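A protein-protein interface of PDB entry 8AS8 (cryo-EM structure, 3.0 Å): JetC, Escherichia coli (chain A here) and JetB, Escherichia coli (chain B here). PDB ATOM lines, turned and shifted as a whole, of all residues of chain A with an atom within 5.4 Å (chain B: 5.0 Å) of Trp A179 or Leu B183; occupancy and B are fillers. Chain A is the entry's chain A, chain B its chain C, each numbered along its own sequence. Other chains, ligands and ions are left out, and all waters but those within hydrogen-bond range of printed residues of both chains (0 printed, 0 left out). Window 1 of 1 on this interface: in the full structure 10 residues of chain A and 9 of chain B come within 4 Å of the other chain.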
ATOM      1  N   TRP A 143     -24.347  10.146 -12.025  1.00  0.00           N
ATOM      2  CA  TRP A 143     -23.090   9.502 -12.362  1.00  0.00           C
ATOM      3  C   TRP A 143     -23.340   8.038 -12.685  1.00  0.00           C
ATOM      4  O   TRP A 143     -24.260   7.422 -12.146  1.00  0.00           O
ATOM      5  CB  TRP A 143     -22.100   9.639 -11.210  1.00  0.00           C
ATOM      6  CG  TRP A 143     -22.035  11.032 -10.691  1.00  0.00           C
ATOM      7  CD1 TRP A 143     -22.802  11.573  -9.708  1.00  0.00           C
ATOM      8  CD2 TRP A 143     -21.171  12.078 -11.145  1.00  0.00           C
ATOM      9  NE1 TRP A 143     -22.463  12.886  -9.509  1.00  0.00           N
ATOM     10  CE2 TRP A 143     -21.464  13.221 -10.382  1.00  0.00           C
ATOM     11  CE3 TRP A 143     -20.174  12.156 -12.120  1.00  0.00           C
ATOM     12  CZ2 TRP A 143     -20.797  14.426 -10.562  1.00  0.00           C
ATOM     13  CZ3 TRP A 143     -19.515  13.353 -12.296  1.00  0.00           C
ATOM     14  CH2 TRP A 143     -19.828  14.472 -11.521  1.00  0.00           C
ATOM     15  N   LEU A 144     -22.529   7.486 -13.579  1.00  0.00           N
ATOM     16  CA  LEU A 144     -22.740   6.143 -14.091  1.00  0.00           C
ATOM     17  C   LEU A 144     -21.436   5.365 -14.078  1.00  0.00           C
ATOM     18  O   LEU A 144     -20.387   5.882 -14.468  1.00  0.00           O
ATOM     19  CB  LEU A 144     -23.303   6.183 -15.509  1.00  0.00           C
ATOM     20  CG  LEU A 144     -24.685   6.818 -15.645  1.00  0.00           C
ATOM     21  CD1 LEU A 144     -24.565   8.274 -16.031  1.00  0.00           C
ATOM     22  CD2 LEU A 144     -25.514   6.069 -16.665  1.00  0.00           C
ATOM     23  N   PHE A 145     -21.515   4.120 -13.632  1.00  0.00           N
ATOM     24  CA  PHE A 145     -20.406   3.184 -13.669  1.00  0.00           C
ATOM     25  C   PHE A 145     -20.871   1.959 -14.435  1.00  0.00           C
ATOM     26  O   PHE A 145     -21.989   1.484 -14.231  1.00  0.00           O
ATOM     27  CB  PHE A 145     -19.962   2.805 -12.259  1.00  0.00           C
ATOM     28  CG  PHE A 145     -18.728   1.957 -12.215  1.00  0.00           C
ATOM     29  CD1 PHE A 145     -18.803   0.593 -12.412  1.00  0.00           C
ATOM     30  CD2 PHE A 145     -17.495   2.524 -11.957  1.00  0.00           C
ATOM     31  CE1 PHE A 145     -17.670  -0.187 -12.364  1.00  0.00           C
ATOM     32  CE2 PHE A 145     -16.360   1.746 -11.909  1.00  0.00           C
ATOM     33  CZ  PHE A 145     -16.448   0.390 -12.113  1.00  0.00           C
ATOM     34  N   SER A 146     -20.032   1.456 -15.332  1.00  0.00           N
ATOM     35  CA  SER A 146     -20.467   0.333 -16.143  1.00  0.00           C
ATOM     36  C   SER A 146     -19.282  -0.553 -16.475  1.00  0.00           C
ATOM     37  O   SER A 146     -18.141  -0.097 -16.519  1.00  0.00           O
ATOM     38  CB  SER A 146     -21.145   0.808 -17.430  1.00  0.00           C
ATOM     39  OG  SER A 146     -21.793  -0.265 -18.084  1.00  0.00           O
ATOM     40  N   ASP A 147     -19.570  -1.830 -16.708  1.00  0.00           N
ATOM     41  CA  ASP A 147     -18.600  -2.758 -17.272  1.00  0.00           C
ATOM     42  C   ASP A 147     -19.182  -3.506 -18.464  1.00  0.00           C
ATOM     43  O   ASP A 147     -18.601  -4.492 -18.923  1.00  0.00           O
ATOM     44  CB  ASP A 147     -18.088  -3.723 -16.199  1.00  0.00           C
ATOM     45  CG  ASP A 147     -19.124  -4.749 -15.771  1.00  0.00           C
ATOM     46  OD1 ASP A 147     -18.919  -5.374 -14.710  1.00  0.00           O
ATOM     47  OD2 ASP A 147     -20.140  -4.932 -16.469  1.00  0.00           O
ATOM     48  N   GLU A 172     -31.642   1.557 -15.700  1.00  0.00           N
ATOM     49  CA  GLU A 172     -30.685   1.009 -14.744  1.00  0.00           C
ATOM     50  C   GLU A 172     -31.221  -0.262 -14.103  1.00  0.00           C
ATOM     51  O   GLU A 172     -30.465  -1.209 -13.860  1.00  0.00           O
ATOM     52  CB  GLU A 172     -30.349   2.034 -13.666  1.00  0.00           C
ATOM     53  CG  GLU A 172     -29.504   1.450 -12.547  1.00  0.00           C
ATOM     54  CD  GLU A 172     -29.777   2.092 -11.204  1.00  0.00           C
ATOM     55  OE1 GLU A 172     -28.839   2.178 -10.384  1.00  0.00           O
ATOM     56  OE2 GLU A 172     -30.930   2.510 -10.966  1.00  0.00           O
ATOM     57  N   GLY A 177     -24.841  -4.800 -15.616  1.00  0.00           N
ATOM     58  CA  GLY A 177     -23.544  -4.164 -15.526  1.00  0.00           C
ATOM     59  C   GLY A 177     -23.559  -2.659 -15.428  1.00  0.00           C
ATOM     60  O   GLY A 177     -22.537  -2.028 -15.712  1.00  0.00           O
ATOM     61  N   LEU A 178     -24.680  -2.058 -15.042  1.00  0.00           N
ATOM     62  CA  LEU A 178     -24.796  -0.613 -14.921  1.00  0.00           C
ATOM     63  C   LEU A 178     -25.129  -0.236 -13.485  1.00  0.00           C
ATOM     64  O   LEU A 178     -25.920  -0.912 -12.823  1.00  0.00           O
ATOM     65  CB  LEU A 178     -25.867  -0.064 -15.863  1.00  0.00           C
ATOM     66  CG  LEU A 178     -25.926   1.458 -15.979  1.00  0.00           C
ATOM     67  CD1 LEU A 178     -24.740   1.972 -16.762  1.00  0.00           C
ATOM     68  CD2 LEU A 178     -27.222   1.890 -16.629  1.00  0.00           C
ATOM     69  N   TRP A 179     -24.518   0.847 -13.009  1.00  0.00           N
ATOM     70  CA  TRP A 179     -24.755   1.358 -11.664  1.00  0.00           C
ATOM     71  C   TRP A 179     -24.878   2.870 -11.760  1.00  0.00           C
ATOM     72  O   TRP A 179     -23.906   3.549 -12.102  1.00  0.00           O
ATOM     73  CB  TRP A 179     -23.623   0.969 -10.714  1.00  0.00           C
ATOM     74  CG  TRP A 179     -23.590  -0.480 -10.368  1.00  0.00           C
ATOM     75  CD1 TRP A 179     -24.247  -1.091  -9.345  1.00  0.00           C
ATOM     76  CD2 TRP A 179     -22.853  -1.505 -11.039  1.00  0.00           C
ATOM     77  NE1 TRP A 179     -23.971  -2.434  -9.339  1.00  0.00           N
ATOM     78  CE2 TRP A 179     -23.116  -2.714 -10.371  1.00  0.00           C
ATOM     79  CE3 TRP A 179     -21.999  -1.519 -12.143  1.00  0.00           C
ATOM     80  CZ2 TRP A 179     -22.556  -3.922 -10.768  1.00  0.00           C
ATOM     81  CZ3 TRP A 179     -21.445  -2.717 -12.536  1.00  0.00           C
ATOM     82  CH2 TRP A 179     -21.725  -3.903 -11.851  1.00  0.00           C
ATOM     83  N   THR A 180     -26.057   3.401 -11.458  1.00  0.00           N
ATOM     84  CA  THR A 180     -26.302   4.835 -11.511  1.00  0.00           C
ATOM     85  C   THR A 180     -26.389   5.383 -10.096  1.00  0.00           C
ATOM     86  O   THR A 180     -27.154   4.873  -9.273  1.00  0.00           O
ATOM     87  CB  THR A 180     -27.586   5.146 -12.278  1.00  0.00           C
ATOM     88  OG1 THR A 180     -28.717   4.783 -11.478  1.00  0.00           O
ATOM     89  CG2 THR A 180     -27.626   4.366 -13.575  1.00  0.00           C
ATOM     90  N   TYR A 181     -25.603   6.417  -9.820  1.00  0.00           N
ATOM     91  CA  TYR A 181     -25.573   7.069  -8.521  1.00  0.00           C
ATOM     92  C   TYR A 181     -26.052   8.506  -8.668  1.00  0.00           C
ATOM     93  O   TYR A 181     -25.498   9.256  -9.491  1.00  0.00           O
ATOM     94  CB  TYR A 181     -24.164   7.032  -7.930  1.00  0.00           C
ATOM     95  CG  TYR A 181     -23.571   5.647  -7.860  1.00  0.00           C
ATOM     96  CD1 TYR A 181     -22.912   5.098  -8.947  1.00  0.00           C
ATOM     97  CD2 TYR A 181     -23.669   4.888  -6.705  1.00  0.00           C
ATOM     98  CE1 TYR A 181     -22.368   3.834  -8.886  1.00  0.00           C
ATOM     99  CE2 TYR A 181     -23.128   3.624  -6.635  1.00  0.00           C
ATOM    100  CZ  TYR A 181     -22.480   3.102  -7.728  1.00  0.00           C
ATOM    101  OH  TYR A 181     -21.939   1.841  -7.661  1.00  0.00           O
ATOM    102  N   ARG A 190     -17.416   3.871  -5.282  1.00  0.00           N
ATOM    103  CA  ARG A 190     -17.354   2.727  -6.187  1.00  0.00           C
ATOM    104  C   ARG A 190     -16.064   2.733  -6.994  1.00  0.00           C
ATOM    105  O   ARG A 190     -15.451   1.681  -7.209  1.00  0.00           O
ATOM    106  CB  ARG A 190     -18.564   2.725  -7.116  1.00  0.00           C
ATOM    107  CG  ARG A 190     -18.566   1.584  -8.105  1.00  0.00           C
ATOM    108  CD  ARG A 190     -18.885   0.275  -7.423  1.00  0.00           C
ATOM    109  NE  ARG A 190     -19.713  -0.580  -8.262  1.00  0.00           N
ATOM    110  CZ  ARG A 190     -19.272  -1.660  -8.890  1.00  0.00           C
ATOM    111  NH1 ARG A 190     -18.016  -2.057  -8.780  1.00  0.00           N
ATOM    112  NH2 ARG A 190     -20.113  -2.358  -9.646  1.00  0.00           N
ATOM    113  N   ILE B 158     -25.540  -4.515   2.310  1.00  0.00           N
ATOM    114  CA  ILE B 158     -24.541  -5.256   1.549  1.00  0.00           C
ATOM    115  C   ILE B 158     -23.434  -5.749   2.469  1.00  0.00           C
ATOM    116  O   ILE B 158     -22.916  -6.859   2.301  1.00  0.00           O
ATOM    117  CB  ILE B 158     -23.987  -4.386   0.406  1.00  0.00           C
ATOM    118  CG1 ILE B 158     -25.043  -4.231  -0.685  1.00  0.00           C
ATOM    119  CG2 ILE B 158     -22.715  -4.988  -0.155  1.00  0.00           C
ATOM    120  CD1 ILE B 158     -25.961  -5.422  -0.799  1.00  0.00           C
ATOM    121  N   GLU B 178     -13.354  -7.834  -2.171  1.00  0.00           N
ATOM    122  CA  GLU B 178     -14.541  -8.608  -1.829  1.00  0.00           C
ATOM    123  C   GLU B 178     -15.813  -7.807  -2.058  1.00  0.00           C
ATOM    124  O   GLU B 178     -16.832  -8.374  -2.462  1.00  0.00           O
ATOM    125  CB  GLU B 178     -14.466  -9.097  -0.383  1.00  0.00           C
ATOM    126  CG  GLU B 178     -14.255  -8.013   0.645  1.00  0.00           C
ATOM    127  CD  GLU B 178     -13.599  -8.544   1.904  1.00  0.00           C
ATOM    128  OE1 GLU B 178     -12.445  -9.011   1.823  1.00  0.00           O
ATOM    129  OE2 GLU B 178     -14.240  -8.500   2.974  1.00  0.00           O
ATOM    130  N   ARG B 179     -15.776  -6.496  -1.816  1.00  0.00           N
ATOM    131  CA  ARG B 179     -16.936  -5.668  -2.120  1.00  0.00           C
ATOM    132  C   ARG B 179     -17.243  -5.682  -3.611  1.00  0.00           C
ATOM    133  O   ARG B 179     -18.407  -5.774  -4.011  1.00  0.00           O
ATOM    134  CB  ARG B 179     -16.705  -4.241  -1.631  1.00  0.00           C
ATOM    135  CG  ARG B 179     -17.822  -3.709  -0.760  1.00  0.00           C
ATOM    136  CD  ARG B 179     -17.857  -2.197  -0.775  1.00  0.00           C
ATOM    137  NE  ARG B 179     -16.621  -1.625  -0.259  1.00  0.00           N
ATOM    138  CZ  ARG B 179     -16.291  -1.593   1.025  1.00  0.00           C
ATOM    139  NH1 ARG B 179     -17.085  -2.097   1.954  1.00  0.00           N
ATOM    140  NH2 ARG B 179     -15.136  -1.042   1.384  1.00  0.00           N
ATOM    141  N   THR B 180     -16.211  -5.587  -4.450  1.00  0.00           N
ATOM    142  CA  THR B 180     -16.426  -5.651  -5.891  1.00  0.00           C
ATOM    143  C   THR B 180     -16.993  -7.003  -6.303  1.00  0.00           C
ATOM    144  O   THR B 180     -17.908  -7.078  -7.133  1.00  0.00           O
ATOM    145  CB  THR B 180     -15.120  -5.376  -6.631  1.00  0.00           C
ATOM    146  OG1 THR B 180     -14.516  -4.187  -6.109  1.00  0.00           O
ATOM    147  CG2 THR B 180     -15.378  -5.196  -8.111  1.00  0.00           C
ATOM    148  N   ARG B 181     -16.458  -8.084  -5.735  1.00  0.00           N
ATOM    149  CA  ARG B 181     -16.972  -9.413  -6.044  1.00  0.00           C
ATOM    150  C   ARG B 181     -18.443  -9.528  -5.668  1.00  0.00           C
ATOM    151  O   ARG B 181     -19.265 -10.034  -6.445  1.00  0.00           O
ATOM    152  CB  ARG B 181     -16.142 -10.465  -5.309  1.00  0.00           C
ATOM    153  CG  ARG B 181     -16.521 -11.896  -5.618  1.00  0.00           C
ATOM    154  CD  ARG B 181     -15.718 -12.866  -4.771  1.00  0.00           C
ATOM    155  NE  ARG B 181     -15.746 -12.514  -3.357  1.00  0.00           N
ATOM    156  CZ  ARG B 181     -14.833 -12.892  -2.474  1.00  0.00           C
ATOM    157  NH1 ARG B 181     -13.792 -13.624  -2.829  1.00  0.00           N
ATOM    158  NH2 ARG B 181     -14.968 -12.525  -1.203  1.00  0.00           N
ATOM    159  N   LEU B 182     -18.794  -9.050  -4.472  1.00  0.00           N
ATOM    160  CA  LEU B 182     -20.178  -9.116  -4.024  1.00  0.00           C
ATOM    161  C   LEU B 182     -21.084  -8.278  -4.911  1.00  0.00           C
ATOM    162  O   LEU B 182     -22.207  -8.685  -5.219  1.00  0.00           O
ATOM    163  CB  LEU B 182     -20.282  -8.659  -2.572  1.00  0.00           C
ATOM    164  CG  LEU B 182     -21.703  -8.524  -2.029  1.00  0.00           C
ATOM    165  CD1 LEU B 182     -22.457  -9.825  -2.209  1.00  0.00           C
ATOM    166  CD2 LEU B 182     -21.675  -8.112  -0.573  1.00  0.00           C
ATOM    167  N   LEU B 183     -20.621  -7.095  -5.319  1.00  0.00           N
ATOM    168  CA  LEU B 183     -21.436  -6.254  -6.186  1.00  0.00           C
ATOM    169  C   LEU B 183     -21.669  -6.918  -7.535  1.00  0.00           C
ATOM    170  O   LEU B 183     -22.774  -6.851  -8.082  1.00  0.00           O
ATOM    171  CB  LEU B 183     -20.782  -4.887  -6.362  1.00  0.00           C
ATOM    172  CG  LEU B 183     -20.945  -3.948  -5.169  1.00  0.00           C
ATOM    173  CD1 LEU B 183     -20.193  -2.651  -5.393  1.00  0.00           C
ATOM    174  CD2 LEU B 183     -22.413  -3.680  -4.915  1.00  0.00           C
ATOM    175  N   THR B 184     -20.646  -7.567  -8.089  1.00  0.00           N
ATOM    176  CA  THR B 184     -20.839  -8.281  -9.348  1.00  0.00           C
ATOM    177  C   THR B 184     -21.845  -9.415  -9.193  1.00  0.00           C
ATOM    178  O   THR B 184     -22.731  -9.599 -10.041  1.00  0.00           O
ATOM    179  CB  THR B 184     -19.506  -8.821  -9.859  1.00  0.00           C
ATOM    180  OG1 THR B 184     -18.586  -7.737 -10.031  1.00  0.00           O
ATOM    181  CG2 THR B 184     -19.701  -9.530 -11.185  1.00  0.00           C
ATOM    182  N   LEU B 185     -21.726 -10.190  -8.113  1.00  0.00           N
ATOM    183  CA  LEU B 185     -22.676 -11.276  -7.893  1.00  0.00           C
ATOM    184  C   LEU B 185     -24.092 -10.739  -7.726  1.00  0.00           C
ATOM    185  O   LEU B 185     -25.050 -11.308  -8.264  1.00  0.00           O
ATOM    186  CB  LEU B 185     -22.265 -12.098  -6.675  1.00  0.00           C
ATOM    187  CG  LEU B 185     -21.126 -13.090  -6.895  1.00  0.00           C
ATOM    188  CD1 LEU B 185     -20.679 -13.680  -5.574  1.00  0.00           C
ATOM    189  CD2 LEU B 185     -21.555 -14.179  -7.853  1.00  0.00           C
ATOM    190  N   LEU B 186     -24.242  -9.647  -6.977  1.00  0.00           N
ATOM    191  CA  LEU B 186     -25.557  -9.051  -6.786  1.00  0.00           C
ATOM    192  C   LEU B 186     -26.122  -8.544  -8.102  1.00  0.00           C
ATOM    193  O   LEU B 186     -27.327  -8.641  -8.344  1.00  0.00           O
ATOM    194  CB  LEU B 186     -25.478  -7.918  -5.767  1.00  0.00           C
ATOM    195  CG  LEU B 186     -25.311  -8.354  -4.316  1.00  0.00           C
ATOM    196  CD1 LEU B 186     -25.201  -7.145  -3.415  1.00  0.00           C
ATOM    197  CD2 LEU B 186     -26.470  -9.231  -3.898  1.00  0.00           C
ATOM    198  N   ASP B 187     -25.271  -7.983  -8.959  1.00  0.00           N
ATOM    199  CA  ASP B 187     -25.736  -7.537 -10.265  1.00  0.00           C
ATOM    200  C   ASP B 187     -26.247  -8.708 -11.090  1.00  0.00           C
ATOM    201  O   ASP B 187     -27.295  -8.611 -11.739  1.00  0.00           O
ATOM    202  CB  ASP B 187     -24.613  -6.811 -10.998  1.00  0.00           C
ATOM    203  CG  ASP B 187     -25.069  -6.205 -12.302  1.00  0.00           C
ATOM    204  OD1 ASP B 187     -25.731  -5.149 -12.268  1.00  0.00           O
ATOM    205  OD2 ASP B 187     -24.767  -6.784 -13.364  1.00  0.00           O
ATOM    206  N   PRO B 198     -28.071  -1.888  -5.097  1.00  0.00           N
ATOM    207  CA  PRO B 198     -27.928  -1.212  -3.805  1.00  0.00           C
ATOM    208  C   PRO B 198     -28.383   0.236  -3.891  1.00  0.00           C
ATOM    209  O   PRO B 198     -28.125   0.932  -4.874  1.00  0.00           O
ATOM    210  CB  PRO B 198     -26.427  -1.317  -3.515  1.00  0.00           C
ATOM    211  CG  PRO B 198     -25.979  -2.497  -4.290  1.00  0.00           C
ATOM    212  CD  PRO B 198     -26.822  -2.532  -5.530  1.00  0.00           C
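N of Gly A177 is in hydrogen-bond range of OD2 of Asp B187, at 3.0 Å.
The backbone NH (N) of Asp A147 sits at hydrogen-bond distance from the backbone carbonyl oxygen (O) of Gly A177, 3.1 Å away.
O of Phe A145 lies within hydrogen-bond range of N of Trp A179.
The guanidinium group (NE) of Arg A190 lies within hydrogen-bond range of the side-chain hydroxyl (OH) of Tyr A181, at 3.3 Å.
The side-chain hydroxyl (OG) of Ser A146 is in hydrogen-bond range of the backbone carbonyl oxygen (O) of Gly A177.
Leu B183 touches Trp A179.
Trp A179 touches Asp B187.
Arg A190 touches Leu B183.
Printed residues of chain B within 4 Å of Gly A177: Asp B187.
Printed residues of chain B within 4 Å of Arg A190: Leu B183 (3.6 Å).
Printed residues of chain A within 4 Å of Leu B183: Trp A179 (3.98 Å) and Arg A190 (3.6 Å).
Of the printed residues of chain A, Asp B187 touches Gly A177 and Trp A179.
The nearest printed residue of chain B that does not touch Arg A190 is Thr B180 (4.2 Å).
Among the printed residues, 4 pairs touch across the chains.
Among the printed residues, no Asp or Glu carboxylate lies within 4 Å of a Lys or Arg side-chain nitrogen of the other chain.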
